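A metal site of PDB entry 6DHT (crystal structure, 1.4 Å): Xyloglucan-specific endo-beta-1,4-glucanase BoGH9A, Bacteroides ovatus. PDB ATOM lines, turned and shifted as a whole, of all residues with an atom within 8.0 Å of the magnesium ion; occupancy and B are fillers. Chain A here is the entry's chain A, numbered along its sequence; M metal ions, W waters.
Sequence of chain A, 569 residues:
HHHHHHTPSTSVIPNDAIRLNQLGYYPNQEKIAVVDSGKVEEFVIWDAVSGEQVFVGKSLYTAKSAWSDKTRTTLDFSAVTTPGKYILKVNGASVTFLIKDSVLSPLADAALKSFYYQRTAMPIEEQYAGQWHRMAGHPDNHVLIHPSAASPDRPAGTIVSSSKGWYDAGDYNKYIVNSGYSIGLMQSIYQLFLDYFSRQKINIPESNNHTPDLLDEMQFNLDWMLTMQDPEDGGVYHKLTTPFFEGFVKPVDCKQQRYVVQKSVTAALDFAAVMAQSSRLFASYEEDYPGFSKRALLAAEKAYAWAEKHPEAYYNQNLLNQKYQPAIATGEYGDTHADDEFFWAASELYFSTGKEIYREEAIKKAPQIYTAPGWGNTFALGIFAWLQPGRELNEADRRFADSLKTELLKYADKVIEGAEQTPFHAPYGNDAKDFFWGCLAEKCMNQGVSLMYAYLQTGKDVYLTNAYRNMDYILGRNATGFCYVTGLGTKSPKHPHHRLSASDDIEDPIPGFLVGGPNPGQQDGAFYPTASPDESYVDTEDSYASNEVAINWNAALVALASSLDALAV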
ATOM      1  N   TRP A 132      -3.610  -3.281 -15.304  1.00  0.00           N
ATOM      2  CA  TRP A 132      -2.184  -3.411 -14.982  1.00  0.00           C
ATOM      3  C   TRP A 132      -1.848  -2.814 -13.619  1.00  0.00           C
ATOM      4  O   TRP A 132      -0.950  -1.987 -13.494  1.00  0.00           O
ATOM      5  CB  TRP A 132      -1.302  -2.757 -16.058  1.00  0.00           C
ATOM      6  CG  TRP A 132      -1.600  -3.274 -17.456  1.00  0.00           C
ATOM      7  CD1 TRP A 132      -1.080  -4.369 -18.059  1.00  0.00           C
ATOM      8  CD2 TRP A 132      -2.524  -2.711 -18.385  1.00  0.00           C
ATOM      9  NE1 TRP A 132      -1.606  -4.520 -19.302  1.00  0.00           N
ATOM     10  CE2 TRP A 132      -2.501  -3.503 -19.537  1.00  0.00           C
ATOM     11  CE3 TRP A 132      -3.366  -1.598 -18.361  1.00  0.00           C
ATOM     12  CZ2 TRP A 132      -3.285  -3.227 -20.637  1.00  0.00           C
ATOM     13  CZ3 TRP A 132      -4.141  -1.327 -19.451  1.00  0.00           C
ATOM     14  CH2 TRP A 132      -4.088  -2.122 -20.581  1.00  0.00           C
ATOM     15  N   LYS A 494       3.000  -6.789 -28.905  1.00  0.00           N
ATOM     16  CA  LYS A 494       2.328  -7.498 -27.830  1.00  0.00           C
ATOM     17  C   LYS A 494       3.325  -8.178 -26.871  1.00  0.00           C
ATOM     18  O   LYS A 494       2.926  -8.683 -25.799  1.00  0.00           O
ATOM     19  CB  LYS A 494       1.419  -8.567 -28.452  1.00  0.00           C
ATOM     20  CG  LYS A 494       0.272  -8.014 -29.289  1.00  0.00           C
ATOM     21  CD  LYS A 494      -0.750  -7.292 -28.421  1.00  0.00           C
ATOM     22  CE  LYS A 494      -1.783  -6.546 -29.257  1.00  0.00           C
ATOM     23  NZ  LYS A 494      -2.732  -7.436 -29.959  1.00  0.00           N
ATOM     24  N   HIS A 495       4.610  -8.127 -27.209  1.00  0.00           N
ATOM     25  CA  HIS A 495       5.658  -8.853 -26.467  1.00  0.00           C
ATOM     26  C   HIS A 495       6.888  -8.018 -26.181  1.00  0.00           C
ATOM     27  O   HIS A 495       8.003  -8.441 -26.426  1.00  0.00           O
ATOM     28  CB  HIS A 495       6.036 -10.116 -27.257  1.00  0.00           C
ATOM     29  CG  HIS A 495       4.877 -11.035 -27.466  1.00  0.00           C
ATOM     30  ND1 HIS A 495       4.358 -11.795 -26.450  1.00  0.00           N
ATOM     31  CD2 HIS A 495       4.091 -11.233 -28.541  1.00  0.00           C
ATOM     32  CE1 HIS A 495       3.308 -12.465 -26.906  1.00  0.00           C
ATOM     33  NE2 HIS A 495       3.136 -12.161 -28.172  1.00  0.00           N
ATOM     34  N   PRO A 496       6.708  -6.797 -25.667  1.00  0.00           N
ATOM     35  CA  PRO A 496       7.894  -5.964 -25.443  1.00  0.00           C
ATOM     36  C   PRO A 496       8.894  -6.548 -24.471  1.00  0.00           C
ATOM     37  O   PRO A 496       8.540  -7.281 -23.548  1.00  0.00           O
ATOM     38  CB  PRO A 496       7.290  -4.657 -24.874  1.00  0.00           C
ATOM     39  CG  PRO A 496       5.999  -5.102 -24.249  1.00  0.00           C
ATOM     40  CD  PRO A 496       5.480  -6.168 -25.163  1.00  0.00           C
ATOM     41  N   HIS A 498      10.273  -5.923 -21.631  1.00  0.00           N
ATOM     42  CA  HIS A 498       9.857  -5.031 -20.535  1.00  0.00           C
ATOM     43  C   HIS A 498       9.561  -5.930 -19.362  1.00  0.00           C
ATOM     44  O   HIS A 498       8.573  -6.662 -19.372  1.00  0.00           O
ATOM     45  CB  HIS A 498       8.568  -4.300 -20.971  1.00  0.00           C
ATOM     46  CG  HIS A 498       8.112  -3.235 -20.027  1.00  0.00           C
ATOM     47  ND1 HIS A 498       6.781  -2.860 -19.925  1.00  0.00           N
ATOM     48  CD2 HIS A 498       8.797  -2.394 -19.217  1.00  0.00           C
ATOM     49  CE1 HIS A 498       6.681  -1.864 -19.069  1.00  0.00           C
ATOM     50  NE2 HIS A 498       7.877  -1.568 -18.620  1.00  0.00           N
ATOM     51  N   ARG A 499      10.401  -5.888 -18.338  1.00  0.00           N
ATOM     52  CA  ARG A 499      10.209  -6.806 -17.225  1.00  0.00           C
ATOM     53  C   ARG A 499       8.838  -6.620 -16.558  1.00  0.00           C
ATOM     54  O   ARG A 499       8.234  -7.600 -16.134  1.00  0.00           O
ATOM     55  CB  ARG A 499      11.325  -6.717 -16.204  1.00  0.00           C
ATOM     56  CG  ARG A 499      12.644  -7.389 -16.638  1.00  0.00           C
ATOM     57  CD  ARG A 499      13.760  -7.065 -15.684  1.00  0.00           C
ATOM     58  NE  ARG A 499      15.018  -7.746 -16.029  1.00  0.00           N
ATOM     59  CZ  ARG A 499      15.817  -7.389 -17.024  1.00  0.00           C
ATOM     60  NH1 ARG A 499      15.476  -6.369 -17.818  1.00  0.00           N
ATOM     61  NH2 ARG A 499      16.942  -8.039 -17.236  1.00  0.00           N
ATOM     62  N   LEU A 500       8.319  -5.395 -16.495  1.00  0.00           N
ATOM     63  CA  LEU A 500       6.982  -5.244 -15.904  1.00  0.00           C
ATOM     64  C   LEU A 500       5.891  -5.975 -16.694  1.00  0.00           C
ATOM     65  O   LEU A 500       5.098  -6.706 -16.114  1.00  0.00           O
ATOM     66  CB  LEU A 500       6.596  -3.771 -15.789  1.00  0.00           C
ATOM     67  CG  LEU A 500       7.269  -2.951 -14.687  1.00  0.00           C
ATOM     68  CD1 LEU A 500       6.810  -1.480 -14.780  1.00  0.00           C
ATOM     69  CD2 LEU A 500       7.018  -3.450 -13.301  1.00  0.00           C
ATOM     70  N   SER A 501       5.820  -5.754 -17.999  1.00  0.00           N
ATOM     71  CA  SER A 501       4.792  -6.412 -18.810  1.00  0.00           C
ATOM     72  C   SER A 501       5.006  -7.936 -18.868  1.00  0.00           C
ATOM     73  O   SER A 501       4.047  -8.699 -19.028  1.00  0.00           O
ATOM     74  CB  SER A 501       4.758  -5.870 -20.234  1.00  0.00           C
ATOM     75  OG  SER A 501       4.330  -4.502 -20.243  1.00  0.00           O
ATOM     76  N   ALA A 502       6.269  -8.365 -18.805  1.00  0.00           N
ATOM     77  CA  ALA A 502       6.583  -9.772 -19.025  1.00  0.00           C
ATOM     78  C   ALA A 502       6.327 -10.589 -17.777  1.00  0.00           C
ATOM     79  O   ALA A 502       6.087 -11.801 -17.876  1.00  0.00           O
ATOM     80  CB  ALA A 502       8.037  -9.928 -19.492  1.00  0.00           C
ATOM     81  N   SER A 503       6.394  -9.974 -16.600  1.00  0.00           N
ATOM     82  CA  SER A 503       6.280 -10.708 -15.347  1.00  0.00           C
ATOM     83  C   SER A 503       4.936 -10.575 -14.668  1.00  0.00           C
ATOM     84  O   SER A 503       4.696 -11.207 -13.647  1.00  0.00           O
ATOM     85  CB  SER A 503       7.371 -10.313 -14.378  1.00  0.00           C
ATOM     86  OG  SER A 503       7.215  -8.959 -13.981  1.00  0.00           O
ATOM     87  N   ASP A 504       4.060  -9.742 -15.210  1.00  0.00           N
ATOM     88  CA  ASP A 504       2.727  -9.664 -14.647  1.00  0.00           C
ATOM     89  C   ASP A 504       2.004 -10.855 -15.212  1.00  0.00           C
ATOM     90  O   ASP A 504       2.577 -11.635 -15.951  1.00  0.00           O
ATOM     91  CB  ASP A 504       2.033  -8.314 -14.911  1.00  0.00           C
ATOM     92  CG  ASP A 504       1.800  -8.019 -16.388  1.00  0.00           C
ATOM     93  OD1 ASP A 504       1.789  -8.932 -17.236  1.00  0.00           O
ATOM     94  OD2 ASP A 504       1.572  -6.836 -16.702  1.00  0.00           O
ATOM     95  N   ASP A 505       0.746 -11.005 -14.864  1.00  0.00           N
ATOM     96  CA  ASP A 505       0.019 -12.157 -15.346  1.00  0.00           C
ATOM     97  C   ASP A 505      -1.079 -11.654 -16.261  1.00  0.00           C
ATOM     98  O   ASP A 505      -2.178 -12.180 -16.275  1.00  0.00           O
ATOM     99  CB  ASP A 505      -0.486 -12.987 -14.165  1.00  0.00           C
ATOM    100  CG  ASP A 505       0.663 -13.470 -13.276  1.00  0.00           C
ATOM    101  OD1 ASP A 505       1.580 -14.154 -13.793  1.00  0.00           O
ATOM    102  OD2 ASP A 505       0.657 -13.156 -12.058  1.00  0.00           O
ATOM    103  N   ILE A 506      -0.732 -10.630 -17.038  1.00  0.00           N
ATOM    104  CA  ILE A 506      -1.657  -9.975 -17.962  1.00  0.00           C
ATOM    105  C   ILE A 506      -1.121 -10.115 -19.375  1.00  0.00           C
ATOM    106  O   ILE A 506       0.041  -9.802 -19.638  1.00  0.00           O
ATOM    107  CB  ILE A 506      -1.829  -8.495 -17.582  1.00  0.00           C
ATOM    108  CG1 ILE A 506      -2.392  -8.400 -16.158  1.00  0.00           C
ATOM    109  CG2 ILE A 506      -2.750  -7.795 -18.568  1.00  0.00           C
ATOM    110  CD1 ILE A 506      -2.120  -7.116 -15.502  1.00  0.00           C
ATOM    111  N   GLU A 507      -1.944 -10.643 -20.264  1.00  0.00           N
ATOM    112  CA  GLU A 507      -1.513 -10.918 -21.638  1.00  0.00           C
ATOM    113  C   GLU A 507      -1.127  -9.610 -22.354  1.00  0.00           C
ATOM    114  O   GLU A 507      -0.038  -9.486 -22.895  1.00  0.00           O
ATOM    115  CB  GLU A 507      -2.616 -11.649 -22.408  1.00  0.00           C
ATOM    116  CG  GLU A 507      -2.286 -11.883 -23.884  1.00  0.00           C
ATOM    117  CD  GLU A 507      -3.332 -12.703 -24.617  1.00  0.00           C
ATOM    118  OE1 GLU A 507      -4.167 -13.357 -23.953  1.00  0.00           O
ATOM    119  OE2 GLU A 507      -3.330 -12.684 -25.863  1.00  0.00           O
ATOM    120  N   ASP A 508      -2.017  -8.628 -22.351  1.00  0.00           N
ATOM    121  CA  ASP A 508      -1.715  -7.395 -23.058  1.00  0.00           C
ATOM    122  C   ASP A 508      -0.607  -6.646 -22.325  1.00  0.00           C
ATOM    123  O   ASP A 508      -0.579  -6.576 -21.103  1.00  0.00           O
ATOM    124  CB  ASP A 508      -2.956  -6.516 -23.146  1.00  0.00           C
ATOM    125  CG  ASP A 508      -3.952  -7.030 -24.146  1.00  0.00           C
ATOM    126  OD1 ASP A 508      -3.564  -7.822 -25.039  1.00  0.00           O
ATOM    127  OD2 ASP A 508      -5.119  -6.629 -24.036  1.00  0.00           O
ATOM    128  N   PRO A 509       0.347  -6.083 -23.097  1.00  0.00           N
ATOM    129  CA  PRO A 509       1.388  -5.297 -22.457  1.00  0.00           C
ATOM    130  C   PRO A 509       0.873  -3.991 -21.837  1.00  0.00           C
ATOM    131  O   PRO A 509      -0.199  -3.503 -22.210  1.00  0.00           O
ATOM    132  CB  PRO A 509       2.329  -4.963 -23.619  1.00  0.00           C
ATOM    133  CG  PRO A 509       1.443  -4.938 -24.799  1.00  0.00           C
ATOM    134  CD  PRO A 509       0.463  -6.058 -24.571  1.00  0.00           C
ATOM    135  N   ILE A 510       1.644  -3.424 -20.913  1.00  0.00           N
ATOM    136  CA  ILE A 510       1.312  -2.113 -20.372  1.00  0.00           C
ATOM    137  C   ILE A 510       1.319  -1.157 -21.564  1.00  0.00           C
ATOM    138  O   ILE A 510       2.248  -1.164 -22.388  1.00  0.00           O
ATOM    139  CB  ILE A 510       2.291  -1.690 -19.280  1.00  0.00           C
ATOM    140  CG1 ILE A 510       2.238  -2.713 -18.129  1.00  0.00           C
ATOM    141  CG2 ILE A 510       1.944  -0.267 -18.762  1.00  0.00           C
ATOM    142  CD1 ILE A 510       3.246  -2.500 -17.023  1.00  0.00           C
ATOM    143  N   GLU A 541       9.775 -10.942 -26.323  1.00  0.00           N
ATOM    144  CA  GLU A 541      10.240 -10.364 -25.073  1.00  0.00           C
ATOM    145  C   GLU A 541      11.755 -10.412 -24.890  1.00  0.00           C
ATOM    146  O   GLU A 541      12.320  -9.666 -24.079  1.00  0.00           O
ATOM    147  CB  GLU A 541       9.590 -11.030 -23.857  1.00  0.00           C
ATOM    148  CG  GLU A 541       8.087 -10.803 -23.673  1.00  0.00           C
ATOM    149  CD  GLU A 541       7.174 -11.708 -24.474  1.00  0.00           C
ATOM    150  OE1 GLU A 541       7.642 -12.430 -25.384  1.00  0.00           O
ATOM    151  OE2 GLU A 541       5.943 -11.674 -24.233  1.00  0.00           O
HETATM  152 MG    MG M   1       2.052  -9.213 -19.288  1.00  0.00          MG
HETATM  153  O   HOH W   1       2.486 -11.174 -18.837  1.00  0.00           O
HETATM  154  O   HOH W   2       1.499  -7.142 -19.390  1.00  0.00           O
HETATM  155  O   HOH W   3       2.355  -9.252 -21.258  1.00  0.00           O
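Water W3 binds the magnesium ion (2.0 Å).
The magnesium ion is bound by water W1 (2.1 Å).
The backbone carbonyl oxygen (O) of Ser 501 is bound to the magnesium ion, 2.1 Å away.
OD1 of Asp 504 is bound to the magnesium ion, 2.1 Å away.
The magnesium ion is bound by O of Ile 506, 2.1 Å away.
The magnesium ion is bound by water W2 (2.1 Å).
Water W2 lies within hydrogen-bond range of OD2 of Asp 504 and O of Asp 508.
OG of Ser 501 lies within hydrogen-bond range of N of Ile 510, 3.0 Å away.
The side-chain hydroxyl (OG) of Ser 501 sits at hydrogen-bond distance from a ring nitrogen (ND1) of His 498, 3.0 Å away.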
